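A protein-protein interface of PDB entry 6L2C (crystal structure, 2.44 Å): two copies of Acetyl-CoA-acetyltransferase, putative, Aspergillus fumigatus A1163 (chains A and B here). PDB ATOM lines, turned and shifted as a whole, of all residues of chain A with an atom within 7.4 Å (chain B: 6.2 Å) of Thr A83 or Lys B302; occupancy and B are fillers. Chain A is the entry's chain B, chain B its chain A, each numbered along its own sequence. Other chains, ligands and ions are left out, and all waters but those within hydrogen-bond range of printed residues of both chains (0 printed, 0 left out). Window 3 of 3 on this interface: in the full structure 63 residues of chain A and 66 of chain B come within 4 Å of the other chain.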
ATOM      1  N   GLU A  51       8.868  24.989 -14.744  1.00  0.00           N
ATOM      2  CA  GLU A  51       8.890  24.593 -13.315  1.00  0.00           C
ATOM      3  C   GLU A  51       7.478  24.570 -12.712  1.00  0.00           C
ATOM      4  O   GLU A  51       7.317  23.940 -11.678  1.00  0.00           O
ATOM      5  CB  GLU A  51       9.798  25.571 -12.576  1.00  0.00           C
ATOM      6  CG  GLU A  51      10.953  26.050 -13.436  1.00  0.00           C
ATOM      7  CD  GLU A  51      10.794  27.428 -14.046  1.00  0.00           C
ATOM      8  OE1 GLU A  51      10.120  28.252 -13.441  1.00  0.00           O
ATOM      9  OE2 GLU A  51      11.364  27.672 -15.104  1.00  0.00           O
ATOM     10  N   ILE A  53       4.708  23.319 -14.309  1.00  0.00           N
ATOM     11  CA  ILE A  53       4.022  22.061 -14.733  1.00  0.00           C
ATOM     12  C   ILE A  53       4.464  20.903 -13.835  1.00  0.00           C
ATOM     13  O   ILE A  53       5.636  20.602 -13.807  1.00  0.00           O
ATOM     14  CB  ILE A  53       4.261  21.784 -16.224  1.00  0.00           C
ATOM     15  CG1 ILE A  53       3.627  22.866 -17.092  1.00  0.00           C
ATOM     16  CG2 ILE A  53       3.752  20.412 -16.598  1.00  0.00           C
ATOM     17  CD1 ILE A  53       4.447  23.258 -18.284  1.00  0.00           C
ATOM     18  N   THR A  54       3.525  20.242 -13.174  1.00  0.00           N
ATOM     19  CA  THR A  54       3.879  19.197 -12.188  1.00  0.00           C
ATOM     20  C   THR A  54       3.355  17.804 -12.548  1.00  0.00           C
ATOM     21  O   THR A  54       3.755  16.872 -11.883  1.00  0.00           O
ATOM     22  CB  THR A  54       3.406  19.602 -10.791  1.00  0.00           C
ATOM     23  OG1 THR A  54       1.998  19.767 -10.826  1.00  0.00           O
ATOM     24  CG2 THR A  54       4.033  20.889 -10.325  1.00  0.00           C
ATOM     25  N   ASP A  55       2.471  17.676 -13.527  1.00  0.00           N
ATOM     26  CA  ASP A  55       1.988  16.326 -13.888  1.00  0.00           C
ATOM     27  C   ASP A  55       1.878  16.219 -15.399  1.00  0.00           C
ATOM     28  O   ASP A  55       1.668  17.215 -16.017  1.00  0.00           O
ATOM     29  CB  ASP A  55       0.620  16.025 -13.287  1.00  0.00           C
ATOM     30  CG  ASP A  55       0.630  15.749 -11.803  1.00  0.00           C
ATOM     31  OD1 ASP A  55       0.499  16.695 -11.044  1.00  0.00           O
ATOM     32  OD2 ASP A  55       0.728  14.594 -11.431  1.00  0.00           O
ATOM     33  N   ARG A  72       5.525   8.565 -18.516  1.00  0.00           N
ATOM     34  CA  ARG A  72       6.827   8.975 -17.960  1.00  0.00           C
ATOM     35  C   ARG A  72       7.853   9.199 -19.038  1.00  0.00           C
ATOM     36  O   ARG A  72       8.590  10.181 -19.012  1.00  0.00           O
ATOM     37  CB  ARG A  72       7.359   7.926 -16.977  1.00  0.00           C
ATOM     38  CG  ARG A  72       8.656   8.264 -16.271  1.00  0.00           C
ATOM     39  CD  ARG A  72       8.612   9.624 -15.591  1.00  0.00           C
ATOM     40  NE  ARG A  72       9.583   9.682 -14.504  1.00  0.00           N
ATOM     41  CZ  ARG A  72       9.886  10.757 -13.788  1.00  0.00           C
ATOM     42  NH1 ARG A  72       9.300  11.934 -14.014  1.00  0.00           N
ATOM     43  NH2 ARG A  72      10.793  10.643 -12.817  1.00  0.00           N
ATOM     44  N   SER A  75       7.083  12.459 -20.959  1.00  0.00           N
ATOM     45  CA  SER A  75       7.491  13.590 -20.178  1.00  0.00           C
ATOM     46  C   SER A  75       9.007  13.754 -20.252  1.00  0.00           C
ATOM     47  O   SER A  75       9.503  14.848 -20.528  1.00  0.00           O
ATOM     48  CB  SER A  75       7.014  13.421 -18.745  1.00  0.00           C
ATOM     49  OG  SER A  75       7.357  14.551 -17.956  1.00  0.00           O
ATOM     50  N   MET A  76       9.728  12.647 -20.068  1.00  0.00           N
ATOM     51  CA  MET A  76      11.164  12.680 -19.907  1.00  0.00           C
ATOM     52  C   MET A  76      11.808  12.979 -21.228  1.00  0.00           C
ATOM     53  O   MET A  76      12.760  13.738 -21.263  1.00  0.00           O
ATOM     54  CB  MET A  76      11.690  11.351 -19.329  1.00  0.00           C
ATOM     55  CG  MET A  76      11.404  11.106 -17.852  1.00  0.00           C
ATOM     56  SD  MET A  76      12.510  12.023 -16.746  1.00  0.00           S
ATOM     57  CE  MET A  76      14.008  11.031 -16.925  1.00  0.00           C
ATOM     58  N   LEU A  80      11.284  17.456 -19.867  1.00  0.00           N
ATOM     59  CA  LEU A  80      10.695  17.871 -18.587  1.00  0.00           C
ATOM     60  C   LEU A  80      11.483  17.209 -17.461  1.00  0.00           C
ATOM     61  O   LEU A  80      12.120  16.171 -17.651  1.00  0.00           O
ATOM     62  CB  LEU A  80       9.181  17.555 -18.521  1.00  0.00           C
ATOM     63  CG  LEU A  80       8.303  18.293 -19.545  1.00  0.00           C
ATOM     64  CD1 LEU A  80       6.817  18.017 -19.395  1.00  0.00           C
ATOM     65  CD2 LEU A  80       8.506  19.793 -19.433  1.00  0.00           C
ATOM     66  N   SER A  81      11.475  17.850 -16.307  1.00  0.00           N
ATOM     67  CA  SER A  81      12.297  17.371 -15.179  1.00  0.00           C
ATOM     68  C   SER A  81      11.745  16.087 -14.580  1.00  0.00           C
ATOM     69  O   SER A  81      10.562  15.856 -14.667  1.00  0.00           O
ATOM     70  CB  SER A  81      12.453  18.454 -14.151  1.00  0.00           C
ATOM     71  OG  SER A  81      11.726  18.174 -12.976  1.00  0.00           O
ATOM     72  N   PRO A  82      12.592  15.273 -13.929  1.00  0.00           N
ATOM     73  CA  PRO A  82      12.169  14.073 -13.213  1.00  0.00           C
ATOM     74  C   PRO A  82      11.233  14.262 -12.009  1.00  0.00           C
ATOM     75  O   PRO A  82      10.673  13.312 -11.596  1.00  0.00           O
ATOM     76  CB  PRO A  82      13.478  13.509 -12.668  1.00  0.00           C
ATOM     77  CG  PRO A  82      14.506  14.024 -13.601  1.00  0.00           C
ATOM     78  CD  PRO A  82      14.031  15.406 -13.956  1.00  0.00           C
ATOM     79  N   THR A  83      11.065  15.484 -11.508  1.00  0.00           N
ATOM     80  CA  THR A  83      10.162  15.809 -10.381  1.00  0.00           C
ATOM     81  C   THR A  83       8.714  15.879 -10.869  1.00  0.00           C
ATOM     82  O   THR A  83       7.839  15.884 -10.031  1.00  0.00           O
ATOM     83  CB  THR A  83      10.595  17.108  -9.707  1.00  0.00           C
ATOM     84  OG1 THR A  83      10.547  18.113 -10.709  1.00  0.00           O
ATOM     85  CG2 THR A  83      12.001  17.041  -9.168  1.00  0.00           C
ATOM     86  N   VAL A  84       8.501  15.950 -12.179  1.00  0.00           N
ATOM     87  CA  VAL A  84       7.149  15.955 -12.796  1.00  0.00           C
ATOM     88  C   VAL A  84       6.554  14.562 -12.635  1.00  0.00           C
ATOM     89  O   VAL A  84       7.210  13.591 -12.980  1.00  0.00           O
ATOM     90  CB  VAL A  84       7.214  16.377 -14.271  1.00  0.00           C
ATOM     91  CG1 VAL A  84       5.860  16.298 -14.929  1.00  0.00           C
ATOM     92  CG2 VAL A  84       7.785  17.765 -14.424  1.00  0.00           C
ATOM     93  N   GLU A  85       5.336  14.498 -12.123  1.00  0.00           N
ATOM     94  CA  GLU A  85       4.683  13.193 -11.913  1.00  0.00           C
ATOM     95  C   GLU A  85       3.956  12.790 -13.186  1.00  0.00           C
ATOM     96  O   GLU A  85       3.694  13.640 -13.997  1.00  0.00           O
ATOM     97  CB  GLU A  85       3.849  13.205 -10.641  1.00  0.00           C
ATOM     98  CG  GLU A  85       4.510  12.429  -9.530  1.00  0.00           C
ATOM     99  CD  GLU A  85       4.513  10.933  -9.758  1.00  0.00           C
ATOM    100  OE1 GLU A  85       4.461  10.200  -8.795  1.00  0.00           O
ATOM    101  OE2 GLU A  85       4.561  10.518 -10.907  1.00  0.00           O
ATOM    102  N   SER A  86       3.678  11.508 -13.341  1.00  0.00           N
ATOM    103  CA  SER A  86       3.036  11.058 -14.592  1.00  0.00           C
ATOM    104  C   SER A  86       2.129   9.864 -14.354  1.00  0.00           C
ATOM    105  O   SER A  86       2.141   9.305 -13.290  1.00  0.00           O
ATOM    106  CB  SER A  86       4.064  10.733 -15.605  1.00  0.00           C
ATOM    107  OG  SER A  86       4.854   9.683 -15.134  1.00  0.00           O
ATOM    108  N   ALA B 287      -0.964  11.962  -1.996  1.00  0.00           N
ATOM    109  CA  ALA B 287       0.137  12.717  -2.590  1.00  0.00           C
ATOM    110  C   ALA B 287       0.927  11.848  -3.562  1.00  0.00           C
ATOM    111  O   ALA B 287       1.165  10.692  -3.282  1.00  0.00           O
ATOM    112  CB  ALA B 287       1.053  13.257  -1.509  1.00  0.00           C
ATOM    113  N   ALA B 289       4.632  11.972  -5.779  1.00  0.00           N
ATOM    114  CA  ALA B 289       5.876  12.710  -5.961  1.00  0.00           C
ATOM    115  C   ALA B 289       6.797  11.893  -6.816  1.00  0.00           C
ATOM    116  O   ALA B 289       6.623  10.667  -6.923  1.00  0.00           O
ATOM    117  CB  ALA B 289       6.526  12.964  -4.625  1.00  0.00           C
ATOM    118  N   ALA B 290       7.801  12.548  -7.385  1.00  0.00           N
ATOM    119  CA  ALA B 290       8.712  11.879  -8.297  1.00  0.00           C
ATOM    120  C   ALA B 290      10.106  12.509  -8.247  1.00  0.00           C
ATOM    121  O   ALA B 290      10.226  13.707  -8.025  1.00  0.00           O
ATOM    122  CB  ALA B 290       8.145  11.924  -9.711  1.00  0.00           C
ATOM    123  N   ILE B 291      11.136  11.677  -8.449  1.00  0.00           N
ATOM    124  CA  ILE B 291      12.535  12.101  -8.495  1.00  0.00           C
ATOM    125  C   ILE B 291      13.174  11.317  -9.649  1.00  0.00           C
ATOM    126  O   ILE B 291      12.443  10.788 -10.473  1.00  0.00           O
ATOM    127  CB  ILE B 291      13.256  11.843  -7.146  1.00  0.00           C
ATOM    128  CG1 ILE B 291      13.261  10.344  -6.810  1.00  0.00           C
ATOM    129  CG2 ILE B 291      12.662  12.694  -6.026  1.00  0.00           C
ATOM    130  CD1 ILE B 291      13.409   9.994  -5.335  1.00  0.00           C
ATOM    131  N   ASP B 292      14.496  11.234  -9.696  1.00  0.00           N
ATOM    132  CA  ASP B 292      15.179  10.531 -10.809  1.00  0.00           C
ATOM    133  C   ASP B 292      14.784   9.061 -10.846  1.00  0.00           C
ATOM    134  O   ASP B 292      14.699   8.457  -9.798  1.00  0.00           O
ATOM    135  CB  ASP B 292      16.695  10.649 -10.724  1.00  0.00           C
ATOM    136  CG  ASP B 292      17.188  12.071 -10.652  1.00  0.00           C
ATOM    137  OD1 ASP B 292      17.103  12.647  -9.582  1.00  0.00           O
ATOM    138  OD2 ASP B 292      17.651  12.575 -11.660  1.00  0.00           O
ATOM    139  N   VAL B 298      13.405   5.596  -3.099  1.00  0.00           N
ATOM    140  CA  VAL B 298      13.233   6.639  -2.045  1.00  0.00           C
ATOM    141  C   VAL B 298      12.155   7.704  -2.358  1.00  0.00           C
ATOM    142  O   VAL B 298      11.924   8.630  -1.565  1.00  0.00           O
ATOM    143  CB  VAL B 298      14.583   7.328  -1.669  1.00  0.00           C
ATOM    144  CG1 VAL B 298      15.507   6.308  -1.018  1.00  0.00           C
ATOM    145  CG2 VAL B 298      15.255   7.978  -2.880  1.00  0.00           C
ATOM    146  N   ALA B 299      11.475   7.558  -3.488  1.00  0.00           N
ATOM    147  CA  ALA B 299      10.377   8.435  -3.805  1.00  0.00           C
ATOM    148  C   ALA B 299       9.288   8.424  -2.716  1.00  0.00           C
ATOM    149  O   ALA B 299       8.687   9.449  -2.456  1.00  0.00           O
ATOM    150  CB  ALA B 299       9.807   8.080  -5.165  1.00  0.00           C
ATOM    151  N   PRO B 300       9.059   7.287  -2.036  1.00  0.00           N
ATOM    152  CA  PRO B 300       8.063   7.330  -0.957  1.00  0.00           C
ATOM    153  C   PRO B 300       8.425   8.260   0.173  1.00  0.00           C
ATOM    154  O   PRO B 300       7.545   8.784   0.832  1.00  0.00           O
ATOM    155  CB  PRO B 300       8.035   5.887  -0.461  1.00  0.00           C
ATOM    156  CG  PRO B 300       8.292   5.109  -1.710  1.00  0.00           C
ATOM    157  CD  PRO B 300       9.417   5.893  -2.361  1.00  0.00           C
ATOM    158  N   ALA B 301       9.714   8.463   0.392  1.00  0.00           N
ATOM    159  CA  ALA B 301      10.175   9.420   1.378  1.00  0.00           C
ATOM    160  C   ALA B 301       9.793  10.839   1.009  1.00  0.00           C
ATOM    161  O   ALA B 301       9.771  11.704   1.875  1.00  0.00           O
ATOM    162  CB  ALA B 301      11.686   9.326   1.542  1.00  0.00           C
ATOM    163  N   LYS B 302       9.561  11.091  -0.278  1.00  0.00           N
ATOM    164  CA  LYS B 302       9.121  12.397  -0.759  1.00  0.00           C
ATOM    165  C   LYS B 302       7.575  12.534  -0.753  1.00  0.00           C
ATOM    166  O   LYS B 302       7.031  13.617  -0.482  1.00  0.00           O
ATOM    167  CB  LYS B 302       9.705  12.658  -2.134  1.00  0.00           C
ATOM    168  CG  LYS B 302       9.419  14.051  -2.656  1.00  0.00           C
ATOM    169  CD  LYS B 302      10.134  14.308  -3.976  1.00  0.00           C
ATOM    170  CE  LYS B 302       9.608  15.576  -4.650  1.00  0.00           C
ATOM    171  NZ  LYS B 302      10.331  15.852  -5.927  1.00  0.00           N
ATOM    172  N   ALA B 303       6.869  11.442  -1.015  1.00  0.00           N
ATOM    173  CA  ALA B 303       5.439  11.518  -1.077  1.00  0.00           C
ATOM    174  C   ALA B 303       4.829  11.638   0.320  1.00  0.00           C
ATOM    175  O   ALA B 303       3.914  12.451   0.504  1.00  0.00           O
ATOM    176  CB  ALA B 303       4.844  10.349  -1.853  1.00  0.00           C
ATOM    177  N   VAL B 304       5.308  10.825   1.246  1.00  0.00           N
ATOM    178  CA  VAL B 304       4.749  10.714   2.622  1.00  0.00           C
ATOM    179  C   VAL B 304       4.658  12.071   3.314  1.00  0.00           C
ATOM    180  O   VAL B 304       3.576  12.423   3.719  1.00  0.00           O
ATOM    181  CB  VAL B 304       5.515   9.650   3.422  1.00  0.00           C
ATOM    182  CG1 VAL B 304       5.532   9.944   4.907  1.00  0.00           C
ATOM    183  CG2 VAL B 304       4.965   8.265   3.140  1.00  0.00           C
ATOM    184  N   PRO B 305       5.734  12.854   3.475  1.00  0.00           N
ATOM    185  CA  PRO B 305       5.626  14.181   4.117  1.00  0.00           C
ATOM    186  C   PRO B 305       4.553  15.085   3.506  1.00  0.00           C
ATOM    187  O   PRO B 305       3.851  15.782   4.252  1.00  0.00           O
ATOM    188  CB  PRO B 305       7.007  14.814   3.874  1.00  0.00           C
ATOM    189  CG  PRO B 305       7.919  13.670   3.678  1.00  0.00           C
ATOM    190  CD  PRO B 305       7.094  12.641   2.951  1.00  0.00           C
ATOM    191  N   ILE B 306       4.428  15.068   2.172  1.00  0.00           N
ATOM    192  CA  ILE B 306       3.454  15.916   1.479  1.00  0.00           C
ATOM    193  C   ILE B 306       2.038  15.460   1.859  1.00  0.00           C
ATOM    194  O   ILE B 306       1.223  16.267   2.313  1.00  0.00           O
ATOM    195  CB  ILE B 306       3.622  15.889  -0.048  1.00  0.00           C
ATOM    196  CG1 ILE B 306       4.986  16.447  -0.473  1.00  0.00           C
ATOM    197  CG2 ILE B 306       2.543  16.724  -0.737  1.00  0.00           C
ATOM    198  CD1 ILE B 306       5.257  16.256  -1.963  1.00  0.00           C
ATOM    199  N   ALA B 307       1.763  14.166   1.695  1.00  0.00           N
ATOM    200  CA  ALA B 307       0.499  13.577   2.157  1.00  0.00           C
ATOM    201  C   ALA B 307       0.164  13.891   3.625  1.00  0.00           C
ATOM    202  O   ALA B 307      -0.983  14.178   3.927  1.00  0.00           O
ATOM    203  CB  ALA B 307       0.483  12.081   1.936  1.00  0.00           C
ATOM    204  N   ASN B 334      13.684   3.769   3.446  1.00  0.00           N
ATOM    205  CA  ASN B 334      12.560   4.649   3.789  1.00  0.00           C
ATOM    206  C   ASN B 334      12.338   4.788   5.313  1.00  0.00           C
ATOM    207  O   ASN B 334      11.960   5.859   5.768  1.00  0.00           O
ATOM    208  CB  ASN B 334      11.272   4.237   3.021  1.00  0.00           C
ATOM    209  CG  ASN B 334      11.332   4.640   1.554  1.00  0.00           C
ATOM    210  OD1 ASN B 334      11.517   5.800   1.260  1.00  0.00           O
ATOM    211  ND2 ASN B 334      11.193   3.690   0.634  1.00  0.00           N
ATOM    212  N   LEU B 338      12.693   8.544   6.902  1.00  0.00           N
ATOM    213  CA  LEU B 338      11.539   9.027   7.611  1.00  0.00           C
ATOM    214  C   LEU B 338      11.599   8.857   9.135  1.00  0.00           C
ATOM    215  O   LEU B 338      10.706   9.379   9.842  1.00  0.00           O
ATOM    216  CB  LEU B 338      10.279   8.329   7.080  1.00  0.00           C
ATOM    217  CG  LEU B 338       9.959   8.611   5.610  1.00  0.00           C
ATOM    218  CD1 LEU B 338       8.822   7.711   5.168  1.00  0.00           C
ATOM    219  CD2 LEU B 338       9.619  10.069   5.371  1.00  0.00           C
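The backbone carbonyl oxygen (O) of Ile B291 is in hydrogen-bond range of the guanidinium group (NH2) of Arg A72 (2.9 Å). O of Pro A82 lies close to O of Ile B291 (3.3 Å). The side-chain carboxylate of Glu A85 lies close to the backbone carbonyl oxygen of Ala B289, at 2.9 Å.
The side-chain amino group (NZ) of Lys B302 is in hydrogen-bond range of the backbone carbonyl oxygen (O) of Ala B290 (3.0 Å). The backbone carbonyl oxygen (O) of Thr A54 lies within hydrogen-bond range of the backbone NH (N) of Glu A85 (2.9 Å). The guanidinium group (NH2) of Arg A72 is in hydrogen-bond range of the backbone carbonyl oxygen (O) of Pro A82, 2.9 Å away. NH1 of Arg A72 lies within hydrogen-bond range of O of Val A84, at 2.9 Å. The side-chain hydroxyl (OG) of Ser A81 sits at hydrogen-bond distance from the side-chain hydroxyl (OG1) of Thr A83 (2.6 Å).
Ala B290 touches Pro A82 (CB to O, 3.4 Å). Pro A82 touches Asp B292 (CB to N, 3.9 Å). Thr A83 touches Ala B290 (CA to O, 3.2 Å). Thr A83 touches Lys B302 (CG2 to NZ, 3.8 Å). Val A84 touches Ala B290. Glu A85 touches Ala B290 (CG to CB, 3.7 Å).
Of the printed residues of chain B, Arg A72 touches Ile B291 (2.9 Å). Of the printed residues of chain B, Pro A82 touches Ala B290, Ile B291 and Asp B292. Of chain B, only Ala B290 (3.2 Å) and Lys B302 (3.8 Å) come within 4 Å of Thr A83. Of the printed residues of chain B, Glu A85 touches Ala B289 (2.9 Å) and Ala B290 (3.7 Å). Printed residues of chain A within 4 Å of Ala B290: Pro A82 (3.4 Å), Thr A83 (3.2 Å), Val A84 (3.8 Å) and Glu A85 (3.7 Å). Printed residues of chain A within 4 Å of Asp B292: Pro A82 (3.9 Å). Ala B301 touches none of the printed residues of chain A. Lys B302 touches just one residue of chain A: Thr A83 (3.8 Å). The nearest printed residue of chain B that does not touch Glu A85 is Ala B287 (6.4 Å).
Hydrophobic or aromatic side chains of chain A that line the printed part of chain B: Pro A82. Along chain B the printed residues that touch a printed residue of chain A span positions 289 to 302. Among the printed residues, no Asp or Glu carboxylate lies within 4 Å of a Lys or Arg side-chain nitrogen of the other chain.
No position is printed for both chains. Of the 9 pairs that touch across the chains among the printed residues, none has its exchanged pair printed and touching as well.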
